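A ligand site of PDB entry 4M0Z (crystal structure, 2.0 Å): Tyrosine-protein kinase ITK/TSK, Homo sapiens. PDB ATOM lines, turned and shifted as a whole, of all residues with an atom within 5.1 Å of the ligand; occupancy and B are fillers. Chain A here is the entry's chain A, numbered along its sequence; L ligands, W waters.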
ATOM      1  N   TRP A   5      10.175  11.602  35.808  1.00  0.00           N
ATOM      2  CA  TRP A   5      10.407  11.429  34.386  1.00  0.00           C
ATOM      3  C   TRP A   5      10.965  12.666  33.652  1.00  0.00           C
ATOM      4  O   TRP A   5      11.476  12.510  32.543  1.00  0.00           O
ATOM      5  CB  TRP A   5       9.105  10.972  33.737  1.00  0.00           C
ATOM      6  CG  TRP A   5       7.963  11.888  34.025  1.00  0.00           C
ATOM      7  CD1 TRP A   5       7.140  11.873  35.124  1.00  0.00           C
ATOM      8  CD2 TRP A   5       7.551  13.007  33.240  1.00  0.00           C
ATOM      9  NE1 TRP A   5       6.228  12.883  35.034  1.00  0.00           N
ATOM     10  CE2 TRP A   5       6.455  13.606  33.900  1.00  0.00           C
ATOM     11  CE3 TRP A   5       7.967  13.522  31.998  1.00  0.00           C
ATOM     12  CZ2 TRP A   5       5.813  14.736  33.386  1.00  0.00           C
ATOM     13  CZ3 TRP A   5       7.318  14.640  31.485  1.00  0.00           C
ATOM     14  CH2 TRP A   5       6.260  15.239  32.183  1.00  0.00           C
ATOM     15  N   PHE A  52       1.242  12.671  25.420  1.00  0.00           N
ATOM     16  CA  PHE A  52       2.349  11.820  25.817  1.00  0.00           C
ATOM     17  C   PHE A  52       2.756  12.083  27.276  1.00  0.00           C
ATOM     18  O   PHE A  52       2.720  11.153  28.086  1.00  0.00           O
ATOM     19  CB  PHE A  52       3.533  12.001  24.841  1.00  0.00           C
ATOM     20  CG  PHE A  52       4.723  11.139  25.154  1.00  0.00           C
ATOM     21  CD1 PHE A  52       4.720   9.774  24.835  1.00  0.00           C
ATOM     22  CD2 PHE A  52       5.849  11.681  25.766  1.00  0.00           C
ATOM     23  CE1 PHE A  52       5.835   8.979  25.123  1.00  0.00           C
ATOM     24  CE2 PHE A  52       6.957  10.881  26.042  1.00  0.00           C
ATOM     25  CZ  PHE A  52       6.937   9.533  25.728  1.00  0.00           C
ATOM     26  N   ILE A  53       3.049  13.353  27.606  1.00  0.00           N
ATOM     27  CA  ILE A  53       3.461  13.837  28.933  1.00  0.00           C
ATOM     28  C   ILE A  53       2.469  13.425  30.041  1.00  0.00           C
ATOM     29  O   ILE A  53       2.899  13.017  31.124  1.00  0.00           O
ATOM     30  CB  ILE A  53       3.699  15.387  28.832  1.00  0.00           C
ATOM     31  CG1 ILE A  53       5.063  15.697  28.195  1.00  0.00           C
ATOM     32  CG2 ILE A  53       3.497  16.140  30.160  1.00  0.00           C
ATOM     33  CD1 ILE A  53       5.111  17.063  27.400  1.00  0.00           C
ATOM     34  N   GLU A  55       0.620  10.773  30.352  1.00  0.00           N
ATOM     35  CA  GLU A  55       0.716   9.353  30.701  1.00  0.00           C
ATOM     36  C   GLU A  55       2.052   8.933  31.312  1.00  0.00           C
ATOM     37  O   GLU A  55       2.193   7.767  31.676  1.00  0.00           O
ATOM     38  CB  GLU A  55       0.423   8.506  29.458  1.00  0.00           C
ATOM     39  CG  GLU A  55      -1.053   8.536  29.056  1.00  0.00           C
ATOM     40  CD  GLU A  55      -1.364   7.784  27.776  1.00  0.00           C
ATOM     41  OE1 GLU A  55      -0.666   6.787  27.490  1.00  0.00           O
ATOM     42  OE2 GLU A  55      -2.298   8.208  27.061  1.00  0.00           O
ATOM     43  N   ALA A  56       3.007   9.865  31.433  1.00  0.00           N
ATOM     44  CA  ALA A  56       4.350   9.605  31.973  1.00  0.00           C
ATOM     45  C   ALA A  56       4.363   9.002  33.357  1.00  0.00           C
ATOM     46  O   ALA A  56       4.998   7.981  33.525  1.00  0.00           O
ATOM     47  CB  ALA A  56       5.204  10.863  31.915  1.00  0.00           C
ATOM     48  N   MET A  59       2.993   5.279  32.955  1.00  0.00           N
ATOM     49  CA  MET A  59       3.845   4.560  32.003  1.00  0.00           C
ATOM     50  C   MET A  59       5.292   4.332  32.426  1.00  0.00           C
ATOM     51  O   MET A  59       5.870   3.333  32.013  1.00  0.00           O
ATOM     52  CB  MET A  59       3.742   5.134  30.575  1.00  0.00           C
ATOM     53  CG  MET A  59       2.349   4.982  29.937  1.00  0.00           C
ATOM     54  SD  MET A  59       1.674   3.288  29.937  1.00  0.00           S
ATOM     55  CE  MET A  59       2.455   2.668  28.586  1.00  0.00           C
ATOM     56  N   MET A  60       5.851   5.253  33.240  1.00  0.00           N
ATOM     57  CA  MET A  60       7.235   5.152  33.705  1.00  0.00           C
ATOM     58  C   MET A  60       7.471   3.958  34.618  1.00  0.00           C
ATOM     59  O   MET A  60       8.607   3.484  34.711  1.00  0.00           O
ATOM     60  CB  MET A  60       7.755   6.471  34.322  1.00  0.00           C
ATOM     61  CG  MET A  60       7.217   6.753  35.728  1.00  0.00           C
ATOM     62  SD  MET A  60       7.569   8.430  36.323  1.00  0.00           S
ATOM     63  CE  MET A  60       9.327   8.313  36.630  1.00  0.00           C
ATOM     64  N   LYS A  61       6.407   3.463  35.280  1.00  0.00           N
ATOM     65  CA  LYS A  61       6.420   2.323  36.190  1.00  0.00           C
ATOM     66  C   LYS A  61       6.642   0.985  35.482  1.00  0.00           C
ATOM     67  O   LYS A  61       7.086   0.043  36.135  1.00  0.00           O
ATOM     68  CB  LYS A  61       5.137   2.297  37.031  1.00  0.00           C
ATOM     69  CG  LYS A  61       5.107   3.397  38.100  1.00  0.00           C
ATOM     70  CD  LYS A  61       3.679   3.786  38.484  1.00  0.00           C
ATOM     71  CE  LYS A  61       3.626   5.063  39.297  1.00  0.00           C
ATOM     72  NZ  LYS A  61       2.255   5.639  39.296  1.00  0.00           N
ATOM     73  N   LEU A  62       6.358   0.887  34.159  1.00  0.00           N
ATOM     74  CA  LEU A  62       6.582  -0.352  33.407  1.00  0.00           C
ATOM     75  C   LEU A  62       8.083  -0.594  33.307  1.00  0.00           C
ATOM     76  O   LEU A  62       8.829   0.294  32.876  1.00  0.00           O
ATOM     77  CB  LEU A  62       5.952  -0.291  32.001  1.00  0.00           C
ATOM     78  CG  LEU A  62       4.454  -0.018  31.932  1.00  0.00           C
ATOM     79  CD1 LEU A  62       4.054   0.356  30.531  1.00  0.00           C
ATOM     80  CD2 LEU A  62       3.656  -1.217  32.395  1.00  0.00           C
ATOM     81  N   VAL A  68      12.819  -2.195  26.500  1.00  0.00           N
ATOM     82  CA  VAL A  68      13.770  -1.071  26.470  1.00  0.00           C
ATOM     83  C   VAL A  68      13.218  -0.033  27.450  1.00  0.00           C
ATOM     84  O   VAL A  68      12.074   0.403  27.288  1.00  0.00           O
ATOM     85  CB  VAL A  68      13.960  -0.443  25.043  1.00  0.00           C
ATOM     86  CG1 VAL A  68      14.882   0.786  25.096  1.00  0.00           C
ATOM     87  CG2 VAL A  68      14.502  -1.476  24.049  1.00  0.00           C
ATOM     88  N   GLN A  69      14.007   0.318  28.461  1.00  0.00           N
ATOM     89  CA  GLN A  69      13.580   1.304  29.454  1.00  0.00           C
ATOM     90  C   GLN A  69      13.632   2.731  28.898  1.00  0.00           C
ATOM     91  O   GLN A  69      14.653   3.141  28.363  1.00  0.00           O
ATOM     92  CB  GLN A  69      14.433   1.216  30.734  1.00  0.00           C
ATOM     93  CG  GLN A  69      13.887   2.022  31.933  1.00  0.00           C
ATOM     94  CD  GLN A  69      12.807   1.334  32.731  1.00  0.00           C
ATOM     95  OE1 GLN A  69      12.953   0.184  33.166  1.00  0.00           O
ATOM     96  NE2 GLN A  69      11.734   2.060  33.028  1.00  0.00           N
ATOM     97  N   LEU A  70      12.514   3.455  29.001  1.00  0.00           N
ATOM     98  CA  LEU A  70      12.479   4.869  28.625  1.00  0.00           C
ATOM     99  C   LEU A  70      12.638   5.603  29.958  1.00  0.00           C
ATOM    100  O   LEU A  70      11.719   5.617  30.776  1.00  0.00           O
ATOM    101  CB  LEU A  70      11.157   5.231  27.921  1.00  0.00           C
ATOM    102  CG  LEU A  70      10.864   6.709  27.596  1.00  0.00           C
ATOM    103  CD1 LEU A  70      11.984   7.386  26.838  1.00  0.00           C
ATOM    104  CD2 LEU A  70       9.576   6.848  26.847  1.00  0.00           C
ATOM    105  N   VAL A  73      11.949  12.202  29.757  1.00  0.00           N
ATOM    106  CA  VAL A  73      11.763  13.177  28.688  1.00  0.00           C
ATOM    107  C   VAL A  73      12.420  14.529  29.041  1.00  0.00           C
ATOM    108  O   VAL A  73      12.228  15.057  30.144  1.00  0.00           O
ATOM    109  CB  VAL A  73      10.243  13.326  28.364  1.00  0.00           C
ATOM    110  CG1 VAL A  73       9.964  14.442  27.350  1.00  0.00           C
ATOM    111  CG2 VAL A  73       9.639  11.997  27.886  1.00  0.00           C
ATOM    112  N   PHE A  84      16.438   6.981  26.464  1.00  0.00           N
ATOM    113  CA  PHE A  84      16.320   5.529  26.536  1.00  0.00           C
ATOM    114  C   PHE A  84      17.571   4.839  27.012  1.00  0.00           C
ATOM    115  O   PHE A  84      18.682   5.338  26.865  1.00  0.00           O
ATOM    116  CB  PHE A  84      16.034   4.934  25.147  1.00  0.00           C
ATOM    117  CG  PHE A  84      14.713   5.290  24.516  1.00  0.00           C
ATOM    118  CD1 PHE A  84      13.586   4.527  24.759  1.00  0.00           C
ATOM    119  CD2 PHE A  84      14.599   6.403  23.691  1.00  0.00           C
ATOM    120  CE1 PHE A  84      12.363   4.860  24.172  1.00  0.00           C
ATOM    121  CE2 PHE A  84      13.381   6.709  23.068  1.00  0.00           C
ATOM    122  CZ  PHE A  84      12.274   5.944  23.325  1.00  0.00           C
ATOM    123  N   VAL A 147      11.670  -5.234  23.588  1.00  0.00           N
ATOM    124  CA  VAL A 147      10.570  -4.564  22.877  1.00  0.00           C
ATOM    125  C   VAL A 147      10.624  -3.058  23.228  1.00  0.00           C
ATOM    126  O   VAL A 147      10.896  -2.701  24.369  1.00  0.00           O
ATOM    127  CB  VAL A 147       9.203  -5.204  23.270  1.00  0.00           C
ATOM    128  CG1 VAL A 147       8.027  -4.454  22.656  1.00  0.00           C
ATOM    129  CG2 VAL A 147       9.158  -6.685  22.876  1.00  0.00           C
ATOM    130  N   SER A 148      10.333  -2.194  22.256  1.00  0.00           N
ATOM    131  CA  SER A 148      10.338  -0.749  22.441  1.00  0.00           C
ATOM    132  C   SER A 148       9.205  -0.097  21.643  1.00  0.00           C
ATOM    133  O   SER A 148       8.605  -0.747  20.805  1.00  0.00           O
ATOM    134  CB  SER A 148      11.681  -0.186  21.971  1.00  0.00           C
ATOM    135  OG  SER A 148      11.814   1.166  22.380  1.00  0.00           O
ATOM    136  N   ASP A 149       8.926   1.208  21.912  1.00  0.00           N
ATOM    137  CA  ASP A 149       7.931   2.065  21.259  1.00  0.00           C
ATOM    138  C   ASP A 149       6.496   1.567  21.412  1.00  0.00           C
ATOM    139  O   ASP A 149       5.648   1.866  20.578  1.00  0.00           O
ATOM    140  CB  ASP A 149       8.294   2.330  19.773  1.00  0.00           C
ATOM    141  CG  ASP A 149       9.576   3.087  19.512  1.00  0.00           C
ATOM    142  OD1 ASP A 149      10.083   3.747  20.443  1.00  0.00           O
ATOM    143  OD2 ASP A 149      10.082   3.012  18.380  1.00  0.00           O
ATOM    144  N   PHE A 150       6.211   0.824  22.485  1.00  0.00           N
ATOM    145  CA  PHE A 150       4.858   0.329  22.727  1.00  0.00           C
ATOM    146  C   PHE A 150       3.952   1.501  23.049  1.00  0.00           C
ATOM    147  O   PHE A 150       4.367   2.418  23.761  1.00  0.00           O
ATOM    148  CB  PHE A 150       4.815  -0.761  23.815  1.00  0.00           C
ATOM    149  CG  PHE A 150       5.764  -0.586  24.966  1.00  0.00           C
ATOM    150  CD1 PHE A 150       5.386   0.144  26.096  1.00  0.00           C
ATOM    151  CD2 PHE A 150       7.052  -1.123  24.924  1.00  0.00           C
ATOM    152  CE1 PHE A 150       6.276   0.314  27.163  1.00  0.00           C
ATOM    153  CE2 PHE A 150       7.941  -0.953  25.991  1.00  0.00           C
ATOM    154  CZ  PHE A 150       7.541  -0.244  27.110  1.00  0.00           C
ATOM    155  N   GLY A 151       2.786   1.521  22.413  1.00  0.00           N
ATOM    156  CA  GLY A 151       1.756   2.542  22.566  1.00  0.00           C
ATOM    157  C   GLY A 151       2.007   3.858  21.829  1.00  0.00           C
ATOM    158  O   GLY A 151       1.138   4.725  21.861  1.00  0.00           O
ATOM    159  N   MET A 152       3.167   4.006  21.152  1.00  0.00           N
ATOM    160  CA  MET A 152       3.591   5.231  20.475  1.00  0.00           C
ATOM    161  C   MET A 152       2.658   5.759  19.375  1.00  0.00           C
ATOM    162  O   MET A 152       2.492   6.978  19.256  1.00  0.00           O
ATOM    163  CB  MET A 152       5.044   5.141  19.994  1.00  0.00           C
ATOM    164  CG  MET A 152       6.056   5.152  21.129  1.00  0.00           C
ATOM    165  SD  MET A 152       5.999   6.605  22.237  1.00  0.00           S
ATOM    166  CE  MET A 152       6.908   7.748  21.269  1.00  0.00           C
ATOM    167  N   ARG A 154      -0.403   5.933  19.358  1.00  0.00           N
ATOM    168  CA  ARG A 154      -1.497   6.702  19.954  1.00  0.00           C
ATOM    169  C   ARG A 154      -1.168   8.205  20.001  1.00  0.00           C
ATOM    170  O   ARG A 154      -2.061   9.011  20.190  1.00  0.00           O
ATOM    171  CB  ARG A 154      -1.811   6.214  21.377  1.00  0.00           C
ATOM    172  CG  ARG A 154      -2.587   4.901  21.407  1.00  0.00           C
ATOM    173  CD  ARG A 154      -3.173   4.567  22.764  1.00  0.00           C
ATOM    174  NE  ARG A 154      -2.160   4.353  23.796  1.00  0.00           N
ATOM    175  CZ  ARG A 154      -1.904   5.201  24.794  1.00  0.00           C
ATOM    176  NH1 ARG A 154      -2.570   6.341  24.891  1.00  0.00           N
ATOM    177  NH2 ARG A 154      -0.981   4.907  25.694  1.00  0.00           N
ATOM    178  N   PHE A 155       0.130   8.565  19.870  1.00  0.00           N
ATOM    179  CA  PHE A 155       0.598   9.946  19.932  1.00  0.00           C
ATOM    180  C   PHE A 155       1.064  10.488  18.583  1.00  0.00           C
ATOM    181  O   PHE A 155       1.224  11.697  18.461  1.00  0.00           O
ATOM    182  CB  PHE A 155       1.696  10.100  21.003  1.00  0.00           C
ATOM    183  CG  PHE A 155       1.311   9.445  22.301  1.00  0.00           C
ATOM    184  CD1 PHE A 155       0.362  10.034  23.147  1.00  0.00           C
ATOM    185  CD2 PHE A 155       1.833   8.210  22.660  1.00  0.00           C
ATOM    186  CE1 PHE A 155      -0.016   9.411  24.329  1.00  0.00           C
ATOM    187  CE2 PHE A 155       1.449   7.598  23.850  1.00  0.00           C
ATOM    188  CZ  PHE A 155       0.512   8.196  24.666  1.00  0.00           C
HETATM  189  N1  LIG L   1       6.578   4.098  27.439  1.00  0.00           N
HETATM  190  N2  LIG L   1       6.939   3.778  28.691  1.00  0.00           N
HETATM  191  C1  LIG L   1       8.128   3.104  28.565  1.00  0.00           C
HETATM  192  C2  LIG L   1       8.499   3.007  27.182  1.00  0.00           C
HETATM  193  C3  LIG L   1       7.474   3.649  26.470  1.00  0.00           C
HETATM  194  N3  LIG L   1       9.653   2.402  26.710  1.00  0.00           N
HETATM  195  C4  LIG L   1       9.963   2.375  25.345  1.00  0.00           C
HETATM  196  N4  LIG L   1      11.173   1.801  24.994  1.00  0.00           N
HETATM  197  O1  LIG L   1       9.213   2.837  24.468  1.00  0.00           O
HETATM  198  C5  LIG L   1       8.880   2.557  29.702  1.00  0.00           C
HETATM  199  N5  LIG L   1       8.274   2.575  30.924  1.00  0.00           N
HETATM  200  O2  LIG L   1      10.019   2.089  29.558  1.00  0.00           O
HETATM  201  C6  LIG L   1       5.354   4.789  27.133  1.00  0.00           C
HETATM  202  C7  LIG L   1       4.434   4.140  26.341  1.00  0.00           C
HETATM  203  C8  LIG L   1       3.219   4.778  26.023  1.00  0.00           C
HETATM  204  C9  LIG L   1       2.967   6.037  26.499  1.00  0.00           C
HETATM  205  C10 LIG L   1       5.141   6.115  27.608  1.00  0.00           C
HETATM  206  C11 LIG L   1       3.928   6.728  27.273  1.00  0.00           C
HETATM  207  C12 LIG L   1       3.658   8.050  27.716  1.00  0.00           C
HETATM  208  C13 LIG L   1       4.565   8.720  28.471  1.00  0.00           C
HETATM  209  C14 LIG L   1       5.796   8.090  28.801  1.00  0.00           C
HETATM  210  C15 LIG L   1       6.097   6.817  28.389  1.00  0.00           C
HETATM  211  O3  LIG L   1       6.611   8.907  29.528  1.00  0.00           O
HETATM  212  C16 LIG L   1       7.717   8.310  30.168  1.00  0.00           C
HETATM  213  O   HOH W   1      10.339  -0.401  30.615  1.00  0.00           O
HETATM  214  O   HOH W   2       8.991   5.225  22.817  1.00  0.00           O
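O of Val 68 is in hydrogen-bond range of N4 of the ligand, 2.8 Å away.
The backbone carbonyl oxygen (O) of Leu 62 lies within hydrogen-bond range of a nitrogen (N5) of the ligand (3.1 Å).
The backbone NH of Leu 70 lies within hydrogen-bond range of an oxygen (O2) of the ligand.
The backbone NH (N) of Asp 149 lies within hydrogen-bond range of an oxygen (O1) of the ligand, at 3.0 Å.
The backbone carbonyl oxygen (O) of Met 59 is in hydrogen-bond range of a nitrogen (N5) of the ligand (2.7 Å).
The side-chain hydroxyl of Ser 148 sits at hydrogen-bond distance from a nitrogen (N4) of the ligand, 2.8 Å away.
The side-chain amide nitrogen (NE2) of Gln 69 sits at hydrogen-bond distance from the backbone carbonyl oxygen (O) of Leu 62, 3.4 Å away.
N of Val 68 is in hydrogen-bond range of O of Val 147 (2.9 Å).
OE1 of Glu 55 lies within salt-bridge range of NH2 of Arg 154, at 2.6 Å.
Merely in contact with the ligand: Phe 52 (3.1 Å), Glu 55 (3.7 Å), Ala 56 (3.4 Å), Met 60 (3.9 Å), Gln 69 (3.6 Å), Phe 84 (3.4 Å), Phe 150 (3.1 Å) and Phe 155 (3.4 Å).
Hydrophobic or aromatic side chains within 4 Å of the ligand: Phe 52, Ala 56, Met 59, Leu 62, Val 68, Leu 70, Phe 84, Phe 150 and Phe 155.
Within 4 Å of the ligand: Phe 52, Glu 55, Ala 56, Met 59, Met 60, Leu 62, Val 68, Gln 69, Leu 70, Phe 84, Ser 148, Asp 149, Phe 150 and Phe 155.
The nearest printed residue that does not touch the ligand is Arg 154 (4.2 Å).
Water W1 lies within hydrogen-bond range of O2 of the ligand (2.7 Å) and O of Leu 62 (2.8 Å).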
